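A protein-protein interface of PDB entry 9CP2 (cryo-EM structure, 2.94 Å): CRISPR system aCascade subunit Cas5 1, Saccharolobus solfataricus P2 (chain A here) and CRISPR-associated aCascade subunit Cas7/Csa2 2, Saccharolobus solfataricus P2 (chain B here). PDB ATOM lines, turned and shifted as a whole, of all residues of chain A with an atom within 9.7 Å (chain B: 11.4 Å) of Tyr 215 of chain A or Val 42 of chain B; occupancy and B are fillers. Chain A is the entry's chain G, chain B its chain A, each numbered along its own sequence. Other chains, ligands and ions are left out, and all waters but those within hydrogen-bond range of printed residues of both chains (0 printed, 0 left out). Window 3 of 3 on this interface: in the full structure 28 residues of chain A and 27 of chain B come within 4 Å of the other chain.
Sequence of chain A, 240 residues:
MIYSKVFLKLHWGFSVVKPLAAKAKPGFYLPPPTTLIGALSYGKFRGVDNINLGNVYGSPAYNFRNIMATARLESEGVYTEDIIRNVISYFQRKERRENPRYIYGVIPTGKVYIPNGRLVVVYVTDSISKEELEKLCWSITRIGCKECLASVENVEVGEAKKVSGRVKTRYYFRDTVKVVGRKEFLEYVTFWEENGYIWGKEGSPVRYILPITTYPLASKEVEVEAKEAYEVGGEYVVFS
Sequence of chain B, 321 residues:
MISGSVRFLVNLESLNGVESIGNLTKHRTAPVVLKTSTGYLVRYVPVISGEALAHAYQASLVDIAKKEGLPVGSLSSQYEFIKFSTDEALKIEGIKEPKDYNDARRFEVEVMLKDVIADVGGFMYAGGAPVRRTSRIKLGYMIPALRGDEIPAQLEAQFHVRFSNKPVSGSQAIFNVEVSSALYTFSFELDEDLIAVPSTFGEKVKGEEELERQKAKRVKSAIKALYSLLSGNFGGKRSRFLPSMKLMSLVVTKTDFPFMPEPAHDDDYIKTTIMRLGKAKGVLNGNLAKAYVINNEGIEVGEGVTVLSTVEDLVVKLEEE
Hydrophobic or aromatic side chains of chain B that line the printed part of chain A: Ala 30, Pro 31, Val 33 and Val 42.
Among the printed residues, no Asp or Glu carboxylate lies within 4 Å of a Lys or Arg side-chain nitrogen of the other chain.
Of chain B, only Val 42 comes within 4 Å of Tyr 215 of chain A.
Val 42 of chain B touches one residue of chain A.
No residue of chain B comes within 4 Å of Thr 213 of chain A.
No residue of chain B comes within 4 Å of Thr 214 of chain A.
No residue of chain B comes within 4 Å of Pro 216 of chain A.
Of the printed residues of chain B, Thr 80 of chain A touches Pro 31.
Printed residues of chain A within 4 Å of Pro 31 of chain B: Thr 80 (3.2 Å) and Tyr 113 (3.5 Å).
Gly 77 of chain A touches none of the printed residues of chain B.
Lys 220 of chain A touches none of the printed residues of chain B.
The nearest residue of chain A that does not touch Val 42 of chain B is Val 78 of chain A (5.0 Å).
Among the printed residues, pairs that only touch across the chains: Glu 76 of chain A with Val 33 of chain B (3.6 Å), Val 78 of chain A with Val 33 of chain B (3.5 Å), Thr 80 of chain A with Pro 31 of chain B (3.2 Å), Tyr 113 of chain A with Ala 30 of chain B (3.4 Å), Tyr 113 of chain A with Pro 31 of chain B (3.5 Å) and Tyr 215 of chain A with Val 42 of chain B (3.3 Å).
O of Ala 30 of chain B sits at hydrogen-bond distance from N of Val 45 of chain B (2.9 Å).
O of Val 78 of chain A is in hydrogen-bond range of N of Tyr 113 of chain A (2.9 Å).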
ATOM      1  N   TYR A  29      35.062   8.118  -5.616  1.00  0.00           N
ATOM      2  CA  TYR A  29      33.856   7.377  -5.266  1.00  0.00           C
ATOM      3  C   TYR A  29      32.710   7.703  -6.217  1.00  0.00           C
ATOM      4  O   TYR A  29      31.957   6.810  -6.622  1.00  0.00           O
ATOM      5  CB  TYR A  29      33.462   7.676  -3.820  1.00  0.00           C
ATOM      6  CG  TYR A  29      34.204   6.839  -2.806  1.00  0.00           C
ATOM      7  CD1 TYR A  29      34.286   5.461  -2.940  1.00  0.00           C
ATOM      8  CD2 TYR A  29      34.836   7.431  -1.723  1.00  0.00           C
ATOM      9  CE1 TYR A  29      34.967   4.696  -2.016  1.00  0.00           C
ATOM     10  CE2 TYR A  29      35.521   6.674  -0.796  1.00  0.00           C
ATOM     11  CZ  TYR A  29      35.585   5.308  -0.948  1.00  0.00           C
ATOM     12  OH  TYR A  29      36.268   4.553  -0.023  1.00  0.00           O
ATOM     13  N   GLU A  76      24.024  -0.331  -4.514  1.00  0.00           N
ATOM     14  CA  GLU A  76      25.185  -0.605  -3.678  1.00  0.00           C
ATOM     15  C   GLU A  76      26.337  -1.099  -4.543  1.00  0.00           C
ATOM     16  O   GLU A  76      26.165  -2.029  -5.338  1.00  0.00           O
ATOM     17  CB  GLU A  76      24.844  -1.637  -2.602  1.00  0.00           C
ATOM     18  CG  GLU A  76      23.752  -1.191  -1.641  1.00  0.00           C
ATOM     19  CD  GLU A  76      23.208  -2.334  -0.806  1.00  0.00           C
ATOM     20  OE1 GLU A  76      23.482  -3.504  -1.146  1.00  0.00           O
ATOM     21  OE2 GLU A  76      22.505  -2.063   0.190  1.00  0.00           O
ATOM     22  N   GLY A  77      27.508  -0.478  -4.381  1.00  0.00           N
ATOM     23  CA  GLY A  77      28.693  -0.852  -5.124  1.00  0.00           C
ATOM     24  C   GLY A  77      29.904  -0.940  -4.210  1.00  0.00           C
ATOM     25  O   GLY A  77      29.826  -0.642  -3.018  1.00  0.00           O
ATOM     26  N   VAL A  78      31.025  -1.364  -4.797  1.00  0.00           N
ATOM     27  CA  VAL A  78      32.263  -1.568  -4.048  1.00  0.00           C
ATOM     28  C   VAL A  78      33.407  -0.848  -4.748  1.00  0.00           C
ATOM     29  O   VAL A  78      33.573  -0.974  -5.965  1.00  0.00           O
ATOM     30  CB  VAL A  78      32.606  -3.063  -3.889  1.00  0.00           C
ATOM     31  CG1 VAL A  78      33.826  -3.232  -3.004  1.00  0.00           C
ATOM     32  CG2 VAL A  78      31.437  -3.819  -3.309  1.00  0.00           C
ATOM     33  N   TYR A  79      34.209  -0.118  -3.978  1.00  0.00           N
ATOM     34  CA  TYR A  79      35.416   0.508  -4.498  1.00  0.00           C
ATOM     35  C   TYR A  79      36.576  -0.470  -4.380  1.00  0.00           C
ATOM     36  O   TYR A  79      36.729  -1.139  -3.354  1.00  0.00           O
ATOM     37  CB  TYR A  79      35.725   1.796  -3.737  1.00  0.00           C
ATOM     38  CG  TYR A  79      37.085   2.387  -4.029  1.00  0.00           C
ATOM     39  CD1 TYR A  79      37.294   3.168  -5.154  1.00  0.00           C
ATOM     40  CD2 TYR A  79      38.153   2.179  -3.169  1.00  0.00           C
ATOM     41  CE1 TYR A  79      38.531   3.717  -5.421  1.00  0.00           C
ATOM     42  CE2 TYR A  79      39.393   2.725  -3.428  1.00  0.00           C
ATOM     43  CZ  TYR A  79      39.575   3.492  -4.555  1.00  0.00           C
ATOM     44  OH  TYR A  79      40.808   4.040  -4.820  1.00  0.00           O
ATOM     45  N   THR A  80      37.390  -0.554  -5.430  1.00  0.00           N
ATOM     46  CA  THR A  80      38.472  -1.527  -5.500  1.00  0.00           C
ATOM     47  C   THR A  80      39.721  -0.880  -6.082  1.00  0.00           C
ATOM     48  O   THR A  80      39.635  -0.054  -6.995  1.00  0.00           O
ATOM     49  CB  THR A  80      38.062  -2.738  -6.355  1.00  0.00           C
ATOM     50  OG1 THR A  80      36.844  -3.292  -5.844  1.00  0.00           O
ATOM     51  CG2 THR A  80      39.137  -3.811  -6.328  1.00  0.00           C
ATOM     52  N   TYR A 113      32.979  -0.920  -8.779  1.00  0.00           N
ATOM     53  CA  TYR A 113      32.176  -1.986  -9.354  1.00  0.00           C
ATOM     54  C   TYR A 113      30.739  -1.849  -8.871  1.00  0.00           C
ATOM     55  O   TYR A 113      30.470  -1.909  -7.663  1.00  0.00           O
ATOM     56  CB  TYR A 113      32.756  -3.348  -8.987  1.00  0.00           C
ATOM     57  CG  TYR A 113      33.967  -3.711  -9.813  1.00  0.00           C
ATOM     58  CD1 TYR A 113      33.829  -4.361 -11.031  1.00  0.00           C
ATOM     59  CD2 TYR A 113      35.246  -3.385  -9.385  1.00  0.00           C
ATOM     60  CE1 TYR A 113      34.931  -4.684 -11.797  1.00  0.00           C
ATOM     61  CE2 TYR A 113      36.355  -3.707 -10.141  1.00  0.00           C
ATOM     62  CZ  TYR A 113      36.191  -4.357 -11.345  1.00  0.00           C
ATOM     63  OH  TYR A 113      37.294  -4.678 -12.099  1.00  0.00           O
ATOM     64  N   PHE A 185      27.561  10.883   8.116  1.00  0.00           N
ATOM     65  CA  PHE A 185      27.629  10.316   6.773  1.00  0.00           C
ATOM     66  C   PHE A 185      28.261  11.307   5.808  1.00  0.00           C
ATOM     67  O   PHE A 185      27.752  11.556   4.715  1.00  0.00           O
ATOM     68  CB  PHE A 185      26.244   9.904   6.288  1.00  0.00           C
ATOM     69  CG  PHE A 185      25.596   8.848   7.131  1.00  0.00           C
ATOM     70  CD1 PHE A 185      26.180   7.602   7.273  1.00  0.00           C
ATOM     71  CD2 PHE A 185      24.403   9.101   7.783  1.00  0.00           C
ATOM     72  CE1 PHE A 185      25.585   6.628   8.048  1.00  0.00           C
ATOM     73  CE2 PHE A 185      23.802   8.132   8.560  1.00  0.00           C
ATOM     74  CZ  PHE A 185      24.394   6.893   8.693  1.00  0.00           C
ATOM     75  N   GLU A 187      31.601  12.482   3.591  1.00  0.00           N
ATOM     76  CA  GLU A 187      32.891  12.216   2.970  1.00  0.00           C
ATOM     77  C   GLU A 187      33.377  13.482   2.284  1.00  0.00           C
ATOM     78  O   GLU A 187      32.576  14.258   1.758  1.00  0.00           O
ATOM     79  CB  GLU A 187      32.806  11.078   1.952  1.00  0.00           C
ATOM     80  CG  GLU A 187      32.093   9.840   2.446  1.00  0.00           C
ATOM     81  CD  GLU A 187      32.170   8.703   1.449  1.00  0.00           C
ATOM     82  OE1 GLU A 187      32.727   8.914   0.352  1.00  0.00           O
ATOM     83  OE2 GLU A 187      31.683   7.598   1.765  1.00  0.00           O
ATOM     84  N   ILE A 212      27.682   9.766   1.703  1.00  0.00           N
ATOM     85  CA  ILE A 212      27.959   8.436   1.175  1.00  0.00           C
ATOM     86  C   ILE A 212      28.498   7.550   2.290  1.00  0.00           C
ATOM     87  O   ILE A 212      29.272   8.006   3.138  1.00  0.00           O
ATOM     88  CB  ILE A 212      28.956   8.503  -0.002  1.00  0.00           C
ATOM     89  CG1 ILE A 212      28.373   9.324  -1.153  1.00  0.00           C
ATOM     90  CG2 ILE A 212      29.320   7.114  -0.494  1.00  0.00           C
ATOM     91  CD1 ILE A 212      27.172   8.684  -1.809  1.00  0.00           C
ATOM     92  N   THR A 213      28.077   6.286   2.291  1.00  0.00           N
ATOM     93  CA  THR A 213      28.638   5.273   3.175  1.00  0.00           C
ATOM     94  C   THR A 213      29.815   4.594   2.486  1.00  0.00           C
ATOM     95  O   THR A 213      29.711   4.162   1.335  1.00  0.00           O
ATOM     96  CB  THR A 213      27.583   4.234   3.551  1.00  0.00           C
ATOM     97  OG1 THR A 213      27.108   3.586   2.366  1.00  0.00           O
ATOM     98  CG2 THR A 213      26.415   4.900   4.257  1.00  0.00           C
ATOM     99  N   THR A 214      30.938   4.498   3.203  1.00  0.00           N
ATOM    100  CA  THR A 214      32.190   4.097   2.565  1.00  0.00           C
ATOM    101  C   THR A 214      32.158   2.645   2.087  1.00  0.00           C
ATOM    102  O   THR A 214      32.664   2.340   1.002  1.00  0.00           O
ATOM    103  CB  THR A 214      33.369   4.346   3.513  1.00  0.00           C
ATOM    104  OG1 THR A 214      34.601   4.108   2.821  1.00  0.00           O
ATOM    105  CG2 THR A 214      33.295   3.465   4.754  1.00  0.00           C
ATOM    106  N   TYR A 215      31.572   1.736   2.869  1.00  0.00           N
ATOM    107  CA  TYR A 215      31.574   0.332   2.472  1.00  0.00           C
ATOM    108  C   TYR A 215      30.438  -0.432   3.141  1.00  0.00           C
ATOM    109  O   TYR A 215      30.402  -0.536   4.374  1.00  0.00           O
ATOM    110  CB  TYR A 215      32.917  -0.318   2.812  1.00  0.00           C
ATOM    111  CG  TYR A 215      32.912  -1.830   2.741  1.00  0.00           C
ATOM    112  CD1 TYR A 215      32.537  -2.490   1.578  1.00  0.00           C
ATOM    113  CD2 TYR A 215      33.286  -2.595   3.835  1.00  0.00           C
ATOM    114  CE1 TYR A 215      32.533  -3.869   1.509  1.00  0.00           C
ATOM    115  CE2 TYR A 215      33.284  -3.974   3.775  1.00  0.00           C
ATOM    116  CZ  TYR A 215      32.907  -4.605   2.611  1.00  0.00           C
ATOM    117  OH  TYR A 215      32.904  -5.979   2.545  1.00  0.00           O
ATOM    118  N   PRO A 216      29.494  -0.984   2.370  1.00  0.00           N
ATOM    119  CA  PRO A 216      29.364  -0.894   0.908  1.00  0.00           C
ATOM    120  C   PRO A 216      28.898   0.491   0.478  1.00  0.00           C
ATOM    121  O   PRO A 216      28.315   1.227   1.269  1.00  0.00           O
ATOM    122  CB  PRO A 216      28.332  -1.981   0.585  1.00  0.00           C
ATOM    123  CG  PRO A 216      27.505  -2.093   1.827  1.00  0.00           C
ATOM    124  CD  PRO A 216      28.471  -1.867   2.956  1.00  0.00           C
ATOM    125  N   LEU A 217      29.146   0.872  -0.771  1.00  0.00           N
ATOM    126  CA  LEU A 217      28.879   2.236  -1.204  1.00  0.00           C
ATOM    127  C   LEU A 217      27.380   2.470  -1.342  1.00  0.00           C
ATOM    128  O   LEU A 217      26.667   1.667  -1.951  1.00  0.00           O
ATOM    129  CB  LEU A 217      29.587   2.507  -2.529  1.00  0.00           C
ATOM    130  CG  LEU A 217      29.978   3.952  -2.827  1.00  0.00           C
ATOM    131  CD1 LEU A 217      31.129   4.358  -1.934  1.00  0.00           C
ATOM    132  CD2 LEU A 217      30.364   4.098  -4.284  1.00  0.00           C
ATOM    133  N   ALA A 218      26.904   3.575  -0.773  1.00  0.00           N
ATOM    134  CA  ALA A 218      25.494   3.936  -0.826  1.00  0.00           C
ATOM    135  C   ALA A 218      25.367   5.413  -0.487  1.00  0.00           C
ATOM    136  O   ALA A 218      26.341   6.066  -0.108  1.00  0.00           O
ATOM    137  CB  ALA A 218      24.657   3.076   0.125  1.00  0.00           C
ATOM    138  N   SER A 219      24.150   5.935  -0.625  1.00  0.00           N
ATOM    139  CA  SER A 219      23.872   7.344  -0.388  1.00  0.00           C
ATOM    140  C   SER A 219      22.696   7.494   0.569  1.00  0.00           C
ATOM    141  O   SER A 219      21.715   6.748   0.484  1.00  0.00           O
ATOM    142  CB  SER A 219      23.574   8.077  -1.698  1.00  0.00           C
ATOM    143  OG  SER A 219      22.506   7.457  -2.390  1.00  0.00           O
ATOM    144  N   LYS A 220      22.801   8.466   1.475  1.00  0.00           N
ATOM    145  CA  LYS A 220      21.782   8.726   2.481  1.00  0.00           C
ATOM    146  C   LYS A 220      21.418  10.205   2.473  1.00  0.00           C
ATOM    147  O   LYS A 220      22.219  11.061   2.094  1.00  0.00           O
ATOM    148  CB  LYS A 220      22.257   8.312   3.883  1.00  0.00           C
ATOM    149  CG  LYS A 220      22.958   6.965   3.935  1.00  0.00           C
ATOM    150  CD  LYS A 220      22.000   5.830   3.619  1.00  0.00           C
ATOM    151  CE  LYS A 220      22.735   4.509   3.478  1.00  0.00           C
ATOM    152  NZ  LYS A 220      21.812   3.392   3.136  1.00  0.00           N
ATOM    153  N   THR B  29      39.875 -11.030 -10.618  1.00  0.00           N
ATOM    154  CA  THR B  29      38.562 -11.079  -9.991  1.00  0.00           C
ATOM    155  C   THR B  29      38.149  -9.692  -9.519  1.00  0.00           C
ATOM    156  O   THR B  29      38.977  -8.793  -9.357  1.00  0.00           O
ATOM    157  CB  THR B  29      38.536 -12.053  -8.806  1.00  0.00           C
ATOM    158  OG1 THR B  29      39.644 -11.786  -7.939  1.00  0.00           O
ATOM    159  CG2 THR B  29      38.600 -13.493  -9.288  1.00  0.00           C
ATOM    160  N   ALA B  30      36.846  -9.533  -9.306  1.00  0.00           N
ATOM    161  CA  ALA B  30      36.253  -8.271  -8.898  1.00  0.00           C
ATOM    162  C   ALA B  30      35.186  -8.497  -7.838  1.00  0.00           C
ATOM    163  O   ALA B  30      34.542  -9.549  -7.813  1.00  0.00           O
ATOM    164  CB  ALA B  30      35.632  -7.548 -10.099  1.00  0.00           C
ATOM    165  N   PRO B  31      34.976  -7.523  -6.950  1.00  0.00           N
ATOM    166  CA  PRO B  31      33.963  -7.674  -5.900  1.00  0.00           C
ATOM    167  C   PRO B  31      32.590  -7.180  -6.324  1.00  0.00           C
ATOM    168  O   PRO B  31      32.441  -6.142  -6.971  1.00  0.00           O
ATOM    169  CB  PRO B  31      34.515  -6.808  -4.756  1.00  0.00           C
ATOM    170  CG  PRO B  31      35.860  -6.287  -5.231  1.00  0.00           C
ATOM    171  CD  PRO B  31      35.820  -6.344  -6.714  1.00  0.00           C
ATOM    172  N   VAL B  32      31.567  -7.943  -5.940  1.00  0.00           N
ATOM    173  CA  VAL B  32      30.176  -7.571  -6.156  1.00  0.00           C
ATOM    174  C   VAL B  32      29.409  -7.773  -4.856  1.00  0.00           C
ATOM    175  O   VAL B  32      29.848  -8.488  -3.952  1.00  0.00           O
ATOM    176  CB  VAL B  32      29.512  -8.375  -7.294  1.00  0.00           C
ATOM    177  CG1 VAL B  32      30.216  -8.116  -8.616  1.00  0.00           C
ATOM    178  CG2 VAL B  32      29.498  -9.855  -6.965  1.00  0.00           C
ATOM    179  N   VAL B  33      28.249  -7.126  -4.770  1.00  0.00           N
ATOM    180  CA  VAL B  33      27.370  -7.215  -3.610  1.00  0.00           C
ATOM    181  C   VAL B  33      26.107  -7.960  -4.009  1.00  0.00           C
ATOM    182  O   VAL B  33      25.427  -7.576  -4.968  1.00  0.00           O
ATOM    183  CB  VAL B  33      27.023  -5.827  -3.046  1.00  0.00           C
ATOM    184  CG1 VAL B  33      26.026  -5.959  -1.914  1.00  0.00           C
ATOM    185  CG2 VAL B  33      28.269  -5.140  -2.549  1.00  0.00           C
ATOM    186  N   LEU B  34      25.797  -9.020  -3.273  1.00  0.00           N
ATOM    187  CA  LEU B  34      24.578  -9.792  -3.464  1.00  0.00           C
ATOM    188  C   LEU B  34      23.676  -9.578  -2.257  1.00  0.00           C
ATOM    189  O   LEU B  34      24.094  -9.803  -1.117  1.00  0.00           O
ATOM    190  CB  LEU B  34      24.899 -11.279  -3.651  1.00  0.00           C
ATOM    191  CG  LEU B  34      23.816 -12.201  -4.216  1.00  0.00           C
ATOM    192  CD1 LEU B  34      24.455 -13.368  -4.951  1.00  0.00           C
ATOM    193  CD2 LEU B  34      22.889 -12.712  -3.124  1.00  0.00           C
ATOM    194  N   LYS B  35      22.447  -9.139  -2.510  1.00  0.00           N
ATOM    195  CA  LYS B  35      21.505  -8.834  -1.442  1.00  0.00           C
ATOM    196  C   LYS B  35      20.704 -10.079  -1.086  1.00  0.00           C
ATOM    197  O   LYS B  35      20.225 -10.794  -1.974  1.00  0.00           O
ATOM    198  CB  LYS B  35      20.568  -7.698  -1.855  1.00  0.00           C
ATOM    199  CG  LYS B  35      19.157  -7.823  -1.301  1.00  0.00           C
ATOM    200  CD  LYS B  35      18.336  -6.578  -1.581  1.00  0.00           C
ATOM    201  CE  LYS B  35      16.880  -6.792  -1.207  1.00  0.00           C
ATOM    202  NZ  LYS B  35      16.234  -7.818  -2.071  1.00  0.00           N
ATOM    203  N   THR B  36      20.567 -10.335   0.211  1.00  0.00           N
ATOM    204  CA  THR B  36      19.798 -11.458   0.723  1.00  0.00           C
ATOM    205  C   THR B  36      18.784 -10.946   1.737  1.00  0.00           C
ATOM    206  O   THR B  36      18.830  -9.792   2.169  1.00  0.00           O
ATOM    207  CB  THR B  36      20.704 -12.516   1.370  1.00  0.00           C
ATOM    208  OG1 THR B  36      21.470 -11.915   2.421  1.00  0.00           O
ATOM    209  CG2 THR B  36      21.647 -13.117   0.340  1.00  0.00           C
ATOM    210  N   THR B  38      18.572 -12.031   4.811  1.00  0.00           N
ATOM    211  CA  THR B  38      19.339 -11.802   6.031  1.00  0.00           C
ATOM    212  C   THR B  38      20.130 -10.503   5.954  1.00  0.00           C
ATOM    213  O   THR B  38      20.242  -9.777   6.948  1.00  0.00           O
ATOM    214  CB  THR B  38      20.275 -12.982   6.293  1.00  0.00           C
ATOM    215  OG1 THR B  38      21.209 -13.100   5.213  1.00  0.00           O
ATOM    216  CG2 THR B  38      19.481 -14.274   6.412  1.00  0.00           C
ATOM    217  N   GLY B  39      20.685 -10.192   4.784  1.00  0.00           N
ATOM    218  CA  GLY B  39      21.489  -8.997   4.627  1.00  0.00           C
ATOM    219  C   GLY B  39      22.196  -8.913   3.291  1.00  0.00           C
ATOM    220  O   GLY B  39      21.578  -9.103   2.240  1.00  0.00           O
ATOM    221  N   TYR B  40      23.495  -8.625   3.318  1.00  0.00           N
ATOM    222  CA  TYR B  40      24.286  -8.461   2.110  1.00  0.00           C
ATOM    223  C   TYR B  40      25.538  -9.322   2.190  1.00  0.00           C
ATOM    224  O   TYR B  40      26.030  -9.631   3.277  1.00  0.00           O
ATOM    225  CB  TYR B  40      24.676  -6.993   1.895  1.00  0.00           C
ATOM    226  CG  TYR B  40      25.488  -6.407   3.029  1.00  0.00           C
ATOM    227  CD1 TYR B  40      24.867  -5.795   4.108  1.00  0.00           C
ATOM    228  CD2 TYR B  40      26.876  -6.463   3.017  1.00  0.00           C
ATOM    229  CE1 TYR B  40      25.604  -5.259   5.145  1.00  0.00           C
ATOM    230  CE2 TYR B  40      27.621  -5.930   4.050  1.00  0.00           C
ATOM    231  CZ  TYR B  40      26.980  -5.329   5.111  1.00  0.00           C
ATOM    232  OH  TYR B  40      27.719  -4.796   6.142  1.00  0.00           O
ATOM    233  N   LEU B  41      26.051  -9.703   1.022  1.00  0.00           N
ATOM    234  CA  LEU B  41      27.288 -10.460   0.915  1.00  0.00           C
ATOM    235  C   LEU B  41      28.188  -9.807  -0.119  1.00  0.00           C
ATOM    236  O   LEU B  41      27.707  -9.249  -1.108  1.00  0.00           O
ATOM    237  CB  LEU B  41      27.024 -11.917   0.519  1.00  0.00           C
ATOM    238  CG  LEU B  41      26.067 -12.716   1.401  1.00  0.00           C
ATOM    239  CD1 LEU B  41      25.681 -14.018   0.718  1.00  0.00           C
ATOM    240  CD2 LEU B  41      26.699 -12.985   2.754  1.00  0.00           C
ATOM    241  N   VAL B  42      29.495  -9.884   0.109  1.00  0.00           N
ATOM    242  CA  VAL B  42      30.492  -9.378  -0.825  1.00  0.00           C
ATOM    243  C   VAL B  42      31.186 -10.592  -1.428  1.00  0.00           C
ATOM    244  O   VAL B  42      31.999 -11.251  -0.769  1.00  0.00           O
ATOM    245  CB  VAL B  42      31.491  -8.434  -0.146  1.00  0.00           C
ATOM    246  CG1 VAL B  42      32.636  -8.105  -1.088  1.00  0.00           C
ATOM    247  CG2 VAL B  42      30.791  -7.164   0.302  1.00  0.00           C
ATOM    248  N   ARG B  43      30.864 -10.898  -2.679  1.00  0.00           N
ATOM    249  CA  ARG B  43      31.467 -12.014  -3.388  1.00  0.00           C
ATOM    250  C   ARG B  43      32.586 -11.518  -4.293  1.00  0.00           C
ATOM    251  O   ARG B  43      32.589 -10.367  -4.733  1.00  0.00           O
ATOM    252  CB  ARG B  43      30.429 -12.766  -4.221  1.00  0.00           C
ATOM    253  CG  ARG B  43      29.350 -13.442  -3.406  1.00  0.00           C
ATOM    254  CD  ARG B  43      29.888 -14.687  -2.730  1.00  0.00           C
ATOM    255  NE  ARG B  43      28.857 -15.386  -1.971  1.00  0.00           N
ATOM    256  CZ  ARG B  43      28.038 -16.294  -2.483  1.00  0.00           C
ATOM    257  NH1 ARG B  43      28.105 -16.647  -3.756  1.00  0.00           N
ATOM    258  NH2 ARG B  43      27.130 -16.863  -1.696  1.00  0.00           N
ATOM    259  N   TYR B  44      33.545 -12.400  -4.561  1.00  0.00           N
ATOM    260  CA  TYR B  44      34.632 -12.126  -5.489  1.00  0.00           C
ATOM    261  C   TYR B  44      34.457 -13.033  -6.699  1.00  0.00           C
ATOM    262  O   TYR B  44      34.454 -14.261  -6.561  1.00  0.00           O
ATOM    263  CB  TYR B  44      35.988 -12.347  -4.821  1.00  0.00           C
ATOM    264  CG  TYR B  44      36.481 -11.139  -4.061  1.00  0.00           C
ATOM    265  CD1 TYR B  44      35.848 -10.725  -2.898  1.00  0.00           C
ATOM    266  CD2 TYR B  44      37.570 -10.409  -4.509  1.00  0.00           C
ATOM    267  CE1 TYR B  44      36.292  -9.621  -2.198  1.00  0.00           C
ATOM    268  CE2 TYR B  44      38.021  -9.303  -3.816  1.00  0.00           C
ATOM    269  CZ  TYR B  44      37.379  -8.913  -2.662  1.00  0.00           C
ATOM    270  OH  TYR B  44      37.826  -7.811  -1.971  1.00  0.00           O
ATOM    271  N   VAL B  45      34.320 -12.432  -7.877  1.00  0.00           N
ATOM    272  CA  VAL B  45      33.864 -13.152  -9.063  1.00  0.00           C
ATOM    273  C   VAL B  45      34.855 -12.916 -10.198  1.00  0.00           C
ATOM    274  O   VAL B  45      35.356 -11.792 -10.354  1.00  0.00           O
ATOM    275  CB  VAL B  45      32.442 -12.707  -9.449  1.00  0.00           C
ATOM    276  CG1 VAL B  45      31.906 -13.536 -10.585  1.00  0.00           C
ATOM    277  CG2 VAL B  45      31.510 -12.803  -8.256  1.00  0.00           C
ATOM    278  N   PRO B  46      35.181 -13.936 -10.995  1.00  0.00           N
ATOM    279  CA  PRO B  46      36.158 -13.748 -12.075  1.00  0.00           C
ATOM    280  C   PRO B  46      35.672 -12.788 -13.149  1.00  0.00           C
ATOM    281  O   PRO B  46      34.484 -12.726 -13.474  1.00  0.00           O
ATOM    282  CB  PRO B  46      36.331 -15.163 -12.644  1.00  0.00           C
ATOM    283  CG  PRO B  46      35.123 -15.915 -12.186  1.00  0.00           C
ATOM    284  CD  PRO B  46      34.795 -15.348 -10.849  1.00  0.00           C
ATOM    285  N   LEU B 146      24.871 -10.996 -13.284  1.00  0.00           N
ATOM    286  CA  LEU B 146      24.268 -10.896 -11.955  1.00  0.00           C
ATOM    287  C   LEU B 146      22.748 -10.947 -12.097  1.00  0.00           C
ATOM    288  O   LEU B 146      22.023  -9.981 -11.856  1.00  0.00           O
ATOM    289  CB  LEU B 146      24.726  -9.628 -11.249  1.00  0.00           C
ATOM    290  CG  LEU B 146      26.227  -9.441 -11.040  1.00  0.00           C
ATOM    291  CD1 LEU B 146      26.466  -8.459  -9.913  1.00  0.00           C
ATOM    292  CD2 LEU B 146      26.902 -10.766 -10.736  1.00  0.00           C
ATOM    293  N   ILE B 151      25.032 -16.496  -8.504  1.00  0.00           N
ATOM    294  CA  ILE B 151      26.075 -16.079  -9.434  1.00  0.00           C
ATOM    295  C   ILE B 151      26.675 -17.326 -10.069  1.00  0.00           C
ATOM    296  O   ILE B 151      27.446 -18.041  -9.414  1.00  0.00           O
ATOM    297  CB  ILE B 151      27.154 -15.242  -8.730  1.00  0.00           C
ATOM    298  CG1 ILE B 151      26.540 -13.984  -8.119  1.00  0.00           C
ATOM    299  CG2 ILE B 151      28.249 -14.860  -9.708  1.00  0.00           C
ATOM    300  CD1 ILE B 151      27.527 -13.150  -7.334  1.00  0.00           C
